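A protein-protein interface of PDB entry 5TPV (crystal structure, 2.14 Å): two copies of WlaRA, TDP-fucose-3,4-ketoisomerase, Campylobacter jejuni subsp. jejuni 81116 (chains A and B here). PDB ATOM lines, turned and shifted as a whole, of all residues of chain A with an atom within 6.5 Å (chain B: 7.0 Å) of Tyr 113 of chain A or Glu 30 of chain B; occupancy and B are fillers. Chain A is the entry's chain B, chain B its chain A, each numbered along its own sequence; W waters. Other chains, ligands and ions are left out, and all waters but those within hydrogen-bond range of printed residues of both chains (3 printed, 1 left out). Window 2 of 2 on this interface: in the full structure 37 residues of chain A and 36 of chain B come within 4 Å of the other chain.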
ATOM      1  N   ILE A  31     -30.334  30.917  -9.114  1.00  0.00           N
ATOM      2  CA  ILE A  31     -30.353  30.108 -10.332  1.00  0.00           C
ATOM      3  C   ILE A  31     -29.321  29.003 -10.230  1.00  0.00           C
ATOM      4  O   ILE A  31     -28.244  29.203  -9.734  1.00  0.00           O
ATOM      5  CB  ILE A  31     -30.067  30.911 -11.595  1.00  0.00           C
ATOM      6  CG1 ILE A  31     -31.133  31.995 -11.673  1.00  0.00           C
ATOM      7  CG2 ILE A  31     -30.049  30.021 -12.838  1.00  0.00           C
ATOM      8  CD1 ILE A  31     -30.884  33.122 -12.674  1.00  0.00           C
ATOM      9  N   LYS A  32     -29.738  27.808 -10.627  1.00  0.00           N
ATOM     10  CA  LYS A  32     -28.927  26.590 -10.730  1.00  0.00           C
ATOM     11  C   LYS A  32     -29.065  25.854 -12.111  1.00  0.00           C
ATOM     12  O   LYS A  32     -28.216  25.040 -12.504  1.00  0.00           O
ATOM     13  CB  LYS A  32     -29.507  25.652  -9.677  1.00  0.00           C
ATOM     14  CG  LYS A  32     -28.607  25.064  -8.610  1.00  0.00           C
ATOM     15  CD  LYS A  32     -28.776  25.773  -7.271  1.00  0.00           C
ATOM     16  CE  LYS A  32     -28.493  24.818  -6.117  1.00  0.00           C
ATOM     17  NZ  LYS A  32     -27.422  23.797  -6.357  1.00  0.00           N
ATOM     18  N   ARG A  33     -30.154  26.099 -12.817  1.00  0.00           N
ATOM     19  CA  ARG A  33     -30.440  25.481 -14.089  1.00  0.00           C
ATOM     20  C   ARG A  33     -31.335  26.382 -14.945  1.00  0.00           C
ATOM     21  O   ARG A  33     -32.247  27.086 -14.440  1.00  0.00           O
ATOM     22  CB  ARG A  33     -31.113  24.142 -13.778  1.00  0.00           C
ATOM     23  CG  ARG A  33     -31.962  23.560 -14.897  1.00  0.00           C
ATOM     24  CD  ARG A  33     -32.404  22.121 -14.626  1.00  0.00           C
ATOM     25  NE  ARG A  33     -33.273  22.134 -13.463  1.00  0.00           N
ATOM     26  CZ  ARG A  33     -34.485  21.578 -13.374  1.00  0.00           C
ATOM     27  NH1 ARG A  33     -35.149  21.701 -12.256  1.00  0.00           N
ATOM     28  NH2 ARG A  33     -35.036  20.909 -14.358  1.00  0.00           N
ATOM     29  N   SER A  54     -39.161  23.194  -6.915  1.00  0.00           N
ATOM     30  CA  SER A  54     -38.608  24.200  -7.809  1.00  0.00           C
ATOM     31  C   SER A  54     -39.594  25.349  -7.914  1.00  0.00           C
ATOM     32  O   SER A  54     -40.816  25.172  -8.031  1.00  0.00           O
ATOM     33  CB  SER A  54     -38.381  23.634  -9.211  1.00  0.00           C
ATOM     34  OG  SER A  54     -37.500  22.520  -9.230  1.00  0.00           O
ATOM     35  N   THR A 110     -34.757  28.254 -13.107  1.00  0.00           N
ATOM     36  CA  THR A 110     -35.135  27.559 -11.905  1.00  0.00           C
ATOM     37  C   THR A 110     -33.958  27.432 -10.913  1.00  0.00           C
ATOM     38  O   THR A 110     -32.773  27.644 -11.215  1.00  0.00           O
ATOM     39  CB  THR A 110     -35.771  26.200 -12.209  1.00  0.00           C
ATOM     40  OG1 THR A 110     -36.320  25.590 -11.017  1.00  0.00           O
ATOM     41  CG2 THR A 110     -34.741  25.290 -12.748  1.00  0.00           C
ATOM     42  N   ASN A 111     -34.352  27.169  -9.675  1.00  0.00           N
ATOM     43  CA  ASN A 111     -33.432  27.138  -8.525  1.00  0.00           C
ATOM     44  C   ASN A 111     -33.011  25.730  -8.144  1.00  0.00           C
ATOM     45  O   ASN A 111     -32.424  25.568  -7.106  1.00  0.00           O
ATOM     46  CB  ASN A 111     -34.072  27.837  -7.337  1.00  0.00           C
ATOM     47  CG  ASN A 111     -35.379  27.167  -6.876  1.00  0.00           C
ATOM     48  OD1 ASN A 111     -36.126  26.598  -7.641  1.00  0.00           O
ATOM     49  ND2 ASN A 111     -35.672  27.298  -5.605  1.00  0.00           N
ATOM     50  N   THR A 112     -33.253  24.716  -8.981  1.00  0.00           N
ATOM     51  CA  THR A 112     -32.794  23.371  -8.618  1.00  0.00           C
ATOM     52  C   THR A 112     -32.128  22.653  -9.732  1.00  0.00           C
ATOM     53  O   THR A 112     -32.416  22.943 -10.885  1.00  0.00           O
ATOM     54  CB  THR A 112     -34.009  22.467  -8.238  1.00  0.00           C
ATOM     55  OG1 THR A 112     -34.907  22.391  -9.345  1.00  0.00           O
ATOM     56  CG2 THR A 112     -34.831  23.047  -7.094  1.00  0.00           C
ATOM     57  N   TYR A 113     -31.358  21.613  -9.399  1.00  0.00           N
ATOM     58  CA  TYR A 113     -30.987  20.628 -10.376  1.00  0.00           C
ATOM     59  C   TYR A 113     -32.188  19.792 -10.830  1.00  0.00           C
ATOM     60  O   TYR A 113     -33.114  19.628 -10.071  1.00  0.00           O
ATOM     61  CB  TYR A 113     -29.899  19.704  -9.824  1.00  0.00           C
ATOM     62  CG  TYR A 113     -28.596  20.415  -9.440  1.00  0.00           C
ATOM     63  CD1 TYR A 113     -27.920  21.245 -10.334  1.00  0.00           C
ATOM     64  CD2 TYR A 113     -28.006  20.176  -8.204  1.00  0.00           C
ATOM     65  CE1 TYR A 113     -26.737  21.854 -10.008  1.00  0.00           C
ATOM     66  CE2 TYR A 113     -26.819  20.764  -7.866  1.00  0.00           C
ATOM     67  CZ  TYR A 113     -26.209  21.617  -8.765  1.00  0.00           C
ATOM     68  OH  TYR A 113     -25.037  22.198  -8.400  1.00  0.00           O
ATOM     69  N   TYR A 114     -32.137  19.212 -12.028  1.00  0.00           N
ATOM     70  CA  TYR A 114     -33.239  18.397 -12.499  1.00  0.00           C
ATOM     71  C   TYR A 114     -33.447  17.208 -11.554  1.00  0.00           C
ATOM     72  O   TYR A 114     -32.485  16.592 -11.149  1.00  0.00           O
ATOM     73  CB  TYR A 114     -32.913  17.861 -13.874  1.00  0.00           C
ATOM     74  CG  TYR A 114     -33.884  16.823 -14.302  1.00  0.00           C
ATOM     75  CD1 TYR A 114     -33.502  15.474 -14.393  1.00  0.00           C
ATOM     76  CD2 TYR A 114     -35.195  17.173 -14.593  1.00  0.00           C
ATOM     77  CE1 TYR A 114     -34.421  14.497 -14.720  1.00  0.00           C
ATOM     78  CE2 TYR A 114     -36.119  16.212 -14.945  1.00  0.00           C
ATOM     79  CZ  TYR A 114     -35.716  14.876 -15.000  1.00  0.00           C
ATOM     80  OH  TYR A 114     -36.632  13.938 -15.382  1.00  0.00           O
ATOM     81  N   ASP A 115     -34.690  16.886 -11.216  1.00  0.00           N
ATOM     82  CA  ASP A 115     -34.956  15.786 -10.291  1.00  0.00           C
ATOM     83  C   ASP A 115     -36.327  15.198 -10.581  1.00  0.00           C
ATOM     84  O   ASP A 115     -37.385  15.808 -10.282  1.00  0.00           O
ATOM     85  CB  ASP A 115     -34.905  16.348  -8.905  1.00  0.00           C
ATOM     86  CG  ASP A 115     -35.068  15.289  -7.810  1.00  0.00           C
ATOM     87  OD1 ASP A 115     -35.199  14.057  -8.045  1.00  0.00           O
ATOM     88  OD2 ASP A 115     -35.062  15.787  -6.682  1.00  0.00           O
ATOM     89  N   GLU A 118     -39.167  15.056  -8.075  1.00  0.00           N
ATOM     90  CA  GLU A 118     -39.882  16.216  -7.596  1.00  0.00           C
ATOM     91  C   GLU A 118     -41.146  16.518  -8.329  1.00  0.00           C
ATOM     92  O   GLU A 118     -41.889  17.481  -7.981  1.00  0.00           O
ATOM     93  CB  GLU A 118     -39.023  17.475  -7.417  1.00  0.00           C
ATOM     94  CG  GLU A 118     -38.570  18.116  -8.726  1.00  0.00           C
ATOM     95  CD  GLU A 118     -38.739  19.629  -8.786  1.00  0.00           C
ATOM     96  OE1 GLU A 118     -39.055  20.292  -7.745  1.00  0.00           O
ATOM     97  OE2 GLU A 118     -38.511  20.134  -9.921  1.00  0.00           O
ATOM     98  N   GLN B  22     -27.180  22.825 -16.831  1.00  0.00           N
ATOM     99  CA  GLN B  22     -26.880  22.886 -15.408  1.00  0.00           C
ATOM    100  C   GLN B  22     -25.535  22.237 -15.273  1.00  0.00           C
ATOM    101  O   GLN B  22     -25.053  21.606 -16.180  1.00  0.00           O
ATOM    102  CB  GLN B  22     -27.944  22.181 -14.518  1.00  0.00           C
ATOM    103  CG  GLN B  22     -28.107  20.694 -14.822  1.00  0.00           C
ATOM    104  CD  GLN B  22     -28.997  19.904 -13.840  1.00  0.00           C
ATOM    105  OE1 GLN B  22     -30.163  20.213 -13.602  1.00  0.00           O
ATOM    106  NE2 GLN B  22     -28.448  18.831 -13.326  1.00  0.00           N
ATOM    107  N   LYS B  23     -24.890  22.455 -14.144  1.00  0.00           N
ATOM    108  CA  LYS B  23     -23.640  21.759 -13.850  1.00  0.00           C
ATOM    109  C   LYS B  23     -23.704  20.315 -14.360  1.00  0.00           C
ATOM    110  O   LYS B  23     -24.647  19.613 -14.019  1.00  0.00           O
ATOM    111  CB  LYS B  23     -23.446  21.781 -12.329  1.00  0.00           C
ATOM    112  CG  LYS B  23     -22.365  20.855 -11.827  1.00  0.00           C
ATOM    113  CD  LYS B  23     -21.020  21.211 -12.408  1.00  0.00           C
ATOM    114  CE  LYS B  23     -19.954  20.344 -11.756  1.00  0.00           C
ATOM    115  NZ  LYS B  23     -18.919  21.254 -11.239  1.00  0.00           N
ATOM    116  N   ASP B  24     -22.763  19.915 -15.216  1.00  0.00           N
ATOM    117  CA  ASP B  24     -22.651  18.582 -15.810  1.00  0.00           C
ATOM    118  C   ASP B  24     -23.692  18.189 -16.850  1.00  0.00           C
ATOM    119  O   ASP B  24     -23.611  17.090 -17.371  1.00  0.00           O
ATOM    120  CB  ASP B  24     -22.536  17.489 -14.716  1.00  0.00           C
ATOM    121  CG  ASP B  24     -21.231  17.603 -13.909  1.00  0.00           C
ATOM    122  OD1 ASP B  24     -20.172  17.787 -14.547  1.00  0.00           O
ATOM    123  OD2 ASP B  24     -21.264  17.553 -12.654  1.00  0.00           O
ATOM    124  N   CYS B  27     -22.923  21.902 -19.852  1.00  0.00           N
ATOM    125  CA  CYS B  27     -22.330  22.992 -19.087  1.00  0.00           C
ATOM    126  C   CYS B  27     -21.349  22.386 -18.051  1.00  0.00           C
ATOM    127  O   CYS B  27     -21.755  21.636 -17.145  1.00  0.00           O
ATOM    128  CB  CYS B  27     -23.422  23.787 -18.396  1.00  0.00           C
ATOM    129  SG  CYS B  27     -22.722  25.197 -17.546  1.00  0.00           S
ATOM    130  N   PRO B  28     -20.040  22.659 -18.188  1.00  0.00           N
ATOM    131  CA  PRO B  28     -19.080  22.147 -17.212  1.00  0.00           C
ATOM    132  C   PRO B  28     -19.063  22.843 -15.852  1.00  0.00           C
ATOM    133  O   PRO B  28     -18.468  22.345 -14.927  1.00  0.00           O
ATOM    134  CB  PRO B  28     -17.730  22.319 -17.936  1.00  0.00           C
ATOM    135  CG  PRO B  28     -17.947  23.484 -18.853  1.00  0.00           C
ATOM    136  CD  PRO B  28     -19.415  23.622 -19.104  1.00  0.00           C
ATOM    137  N   PHE B  29     -19.755  23.952 -15.667  1.00  0.00           N
ATOM    138  CA  PHE B  29     -19.691  24.656 -14.415  1.00  0.00           C
ATOM    139  C   PHE B  29     -21.074  24.787 -13.786  1.00  0.00           C
ATOM    140  O   PHE B  29     -22.104  24.483 -14.391  1.00  0.00           O
ATOM    141  CB  PHE B  29     -19.038  26.050 -14.593  1.00  0.00           C
ATOM    142  CG  PHE B  29     -19.606  26.910 -15.712  1.00  0.00           C
ATOM    143  CD1 PHE B  29     -20.808  27.564 -15.585  1.00  0.00           C
ATOM    144  CD2 PHE B  29     -18.902  27.093 -16.884  1.00  0.00           C
ATOM    145  CE1 PHE B  29     -21.304  28.373 -16.599  1.00  0.00           C
ATOM    146  CE2 PHE B  29     -19.387  27.909 -17.899  1.00  0.00           C
ATOM    147  CZ  PHE B  29     -20.594  28.530 -17.761  1.00  0.00           C
ATOM    148  N   GLU B  30     -21.058  25.320 -12.576  1.00  0.00           N
ATOM    149  CA  GLU B  30     -22.223  25.624 -11.811  1.00  0.00           C
ATOM    150  C   GLU B  30     -22.773  26.972 -12.218  1.00  0.00           C
ATOM    151  O   GLU B  30     -22.088  28.030 -12.160  1.00  0.00           O
ATOM    152  CB  GLU B  30     -21.860  25.612 -10.294  1.00  0.00           C
ATOM    153  CG  GLU B  30     -23.059  25.873  -9.369  1.00  0.00           C
ATOM    154  CD  GLU B  30     -24.059  24.692  -9.372  1.00  0.00           C
ATOM    155  OE1 GLU B  30     -25.289  24.867  -9.258  1.00  0.00           O
ATOM    156  OE2 GLU B  30     -23.611  23.543  -9.502  1.00  0.00           O
ATOM    157  N   ILE B  31     -24.031  26.971 -12.610  1.00  0.00           N
ATOM    158  CA  ILE B  31     -24.563  28.194 -13.171  1.00  0.00           C
ATOM    159  C   ILE B  31     -25.041  29.065 -11.983  1.00  0.00           C
ATOM    160  O   ILE B  31     -25.598  28.507 -11.057  1.00  0.00           O
ATOM    161  CB  ILE B  31     -25.731  27.889 -14.120  1.00  0.00           C
ATOM    162  CG1 ILE B  31     -25.274  27.220 -15.412  1.00  0.00           C
ATOM    163  CG2 ILE B  31     -26.469  29.165 -14.467  1.00  0.00           C
ATOM    164  CD1 ILE B  31     -26.421  26.722 -16.293  1.00  0.00           C
ATOM    165  N   LYS B  32     -24.784  30.378 -12.009  1.00  0.00           N
ATOM    166  CA  LYS B  32     -25.288  31.344 -11.023  1.00  0.00           C
ATOM    167  C   LYS B  32     -25.914  32.543 -11.689  1.00  0.00           C
ATOM    168  O   LYS B  32     -26.713  33.253 -11.096  1.00  0.00           O
ATOM    169  CB  LYS B  32     -24.163  31.873 -10.115  1.00  0.00           C
ATOM    170  CG  LYS B  32     -23.513  30.840  -9.200  1.00  0.00           C
ATOM    171  CD  LYS B  32     -23.387  31.340  -7.761  1.00  0.00           C
ATOM    172  CE  LYS B  32     -21.954  31.491  -7.307  1.00  0.00           C
ATOM    173  NZ  LYS B  32     -21.668  32.876  -6.832  1.00  0.00           N
ATOM    174  N   ARG B  33     -25.601  32.781 -12.946  1.00  0.00           N
ATOM    175  CA  ARG B  33     -26.153  33.955 -13.587  1.00  0.00           C
ATOM    176  C   ARG B  33     -26.340  33.672 -15.081  1.00  0.00           C
ATOM    177  O   ARG B  33     -25.534  32.906 -15.636  1.00  0.00           O
ATOM    178  CB  ARG B  33     -25.195  35.140 -13.340  1.00  0.00           C
ATOM    179  CG  ARG B  33     -25.392  36.285 -14.306  1.00  0.00           C
ATOM    180  CD  ARG B  33     -24.584  37.506 -13.842  1.00  0.00           C
ATOM    181  NE  ARG B  33     -23.191  37.156 -13.653  1.00  0.00           N
ATOM    182  CZ  ARG B  33     -22.162  37.763 -14.240  1.00  0.00           C
ATOM    183  NH1 ARG B  33     -20.974  37.262 -13.966  1.00  0.00           N
ATOM    184  NH2 ARG B  33     -22.312  38.809 -15.069  1.00  0.00           N
ATOM    185  N   THR B 110     -23.050  31.887 -17.017  1.00  0.00           N
ATOM    186  CA  THR B 110     -21.810  32.015 -16.214  1.00  0.00           C
ATOM    187  C   THR B 110     -21.975  31.490 -14.784  1.00  0.00           C
ATOM    188  O   THR B 110     -23.103  31.249 -14.341  1.00  0.00           O
ATOM    189  CB  THR B 110     -21.269  33.462 -16.205  1.00  0.00           C
ATOM    190  OG1 THR B 110     -19.920  33.524 -15.672  1.00  0.00           O
ATOM    191  CG2 THR B 110     -22.221  34.409 -15.569  1.00  0.00           C
ATOM    192  N   ASN B 111     -20.815  31.251 -14.177  1.00  0.00           N
ATOM    193  CA  ASN B 111     -20.638  30.754 -12.831  1.00  0.00           C
ATOM    194  C   ASN B 111     -20.393  31.739 -11.682  1.00  0.00           C
ATOM    195  O   ASN B 111     -20.051  31.286 -10.601  1.00  0.00           O
ATOM    196  CB  ASN B 111     -19.548  29.691 -12.798  1.00  0.00           C
ATOM    197  CG  ASN B 111     -18.203  30.235 -13.150  1.00  0.00           C
ATOM    198  OD1 ASN B 111     -18.050  31.262 -13.822  1.00  0.00           O
ATOM    199  ND2 ASN B 111     -17.218  29.426 -12.868  1.00  0.00           N
ATOM    200  N   THR B 112     -20.678  33.023 -11.869  1.00  0.00           N
ATOM    201  CA  THR B 112     -20.412  34.054 -10.873  1.00  0.00           C
ATOM    202  C   THR B 112     -21.509  35.059 -10.877  1.00  0.00           C
ATOM    203  O   THR B 112     -22.141  35.352 -11.911  1.00  0.00           O
ATOM    204  CB  THR B 112     -19.146  34.893 -11.194  1.00  0.00           C
ATOM    205  OG1 THR B 112     -19.255  35.373 -12.550  1.00  0.00           O
ATOM    206  CG2 THR B 112     -17.952  34.041 -11.077  1.00  0.00           C
HETATM  207  O   HOH W   1     -29.942  16.596 -12.155  1.00  0.00           O
HETATM  208  O   HOH W   2     -25.597  24.562 -12.158  1.00  0.00           O
HETATM  209  O   HOH W   3     -28.308  33.284  -8.872  1.00  0.00           O
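Tyr 113 of chain A touches two residues of chain B. Glu 30 of chain B touches just these residues of chain A: Lys 32 (3.4 Å) and Tyr 113 (2.2 Å). Printed residues of chain A within 4 Å of Ile 31 of chain B: Ile 31 (3.0 Å) and Lys 32 (3.9 Å). Of the printed residues of chain A, Gln 22 of chain B touches Lys 32 (3.5 Å), Arg 33 (3.1 Å), Tyr 113 (3.4 Å) and Tyr 114 (2.7 Å). Of the printed residues of chain A, Lys 32 of chain B touches Ile 31 (3.9 Å). Of the printed residues of chain B, Tyr 114 of chain A touches Gln 22 (2.7 Å). Asp 115 of chain A touches none of the printed residues of chain B. The nearest residue of chain B that does not touch Tyr 113 of chain A is Lys 23 of chain B (4.03 Å). The nearest residue of chain A that does not touch Glu 30 of chain B is Ile 31 of chain A (5.3 Å).
Printed residues of chain A that touch a printed residue of chain B: Ile 31, Lys 32, Arg 33, Tyr 113 and Tyr 114. Hydrophobic or aromatic side chains of chain A within 4 Å of the printed part of chain B: Tyr 113 and Tyr 114. Of the 13 printed residues of chain B, 4 touch a printed residue of chain A.
The backbone carbonyl oxygen (O) of Thr 112 of chain A is in hydrogen-bond range of the guanidinium group (NE) of Arg 33 of chain A (2.8 Å). The backbone NH (N) of Lys 32 of chain B sits at hydrogen-bond distance from the backbone carbonyl oxygen (O) of Thr 110 of chain B, 3.0 Å away. N of Lys 32 of chain A lies within hydrogen-bond range of O of Thr 110 of chain A. The backbone NH (N) of Thr 110 of chain A lies within hydrogen-bond range of the backbone carbonyl oxygen (O) of Arg 33 of chain A (3.1 Å).
Water W2 lies within hydrogen-bond range of the backbone carbonyl oxygen of Lys 32 of chain A (2.7 Å), the backbone NH of Ile 31 of chain B (2.9 Å), the side-chain carboxylate of Glu 30 of chain B (2.9 Å) and the backbone NH of Lys 23 of chain B (3.0 Å). Water W1 bridges the backbone carbonyl oxygen (O) of Tyr 114 of chain A and the side-chain amide nitrogen (NE2) of Gln 22 of chain B. Water W3 lies within hydrogen-bond range of O of Lys 32 of chain B (2.7 Å) and N of Ile 31 of chain A (3.1 Å).
Ile 31 of chain A touches its own counterpart, Ile 31 of chain B. Ile 31 of chain A touches Lys 32 of chain B, and with the chains exchanged Lys 32 of chain A touches Ile 31 of chain B. Positions printed for both chains: 31, 32, 33, 110, 111 and 112. Of the 9 pairs that touch across the chains among the printed residues, 3 have their exchanged pair printed and touching as well.
Ile 31 of chain A touches Lys 32 of chain B (O to CA, 3.9 Å). Lys 32 of chain A touches Gln 22 of chain B (O to CB, 3.5 Å). CA of Lys 32 of chain A touches O of Ile 31 of chain B, 3.9 Å away. Arg 33 of chain A touches Gln 22 of chain B. Tyr 113 of chain A touches Gln 22 of chain B (CA to OE1, 3.4 Å).
The side-chain carboxylate of Glu 30 of chain B sits at hydrogen-bond distance from the side-chain hydroxyl of Tyr 113 of chain A (2.8 Å). The side-chain carboxylate of Glu 30 of chain B lies within salt-bridge range of the side-chain amino group of Lys 32 of chain A (3.8 Å). The backbone carbonyl oxygen (O) of Ile 31 of chain A sits close to the backbone carbonyl oxygen (O) of Ile 31 of chain B, at 3.0 Å. OE1 of Gln 22 of chain B is in hydrogen-bond range of N of Tyr 114 of chain A (2.7 Å).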
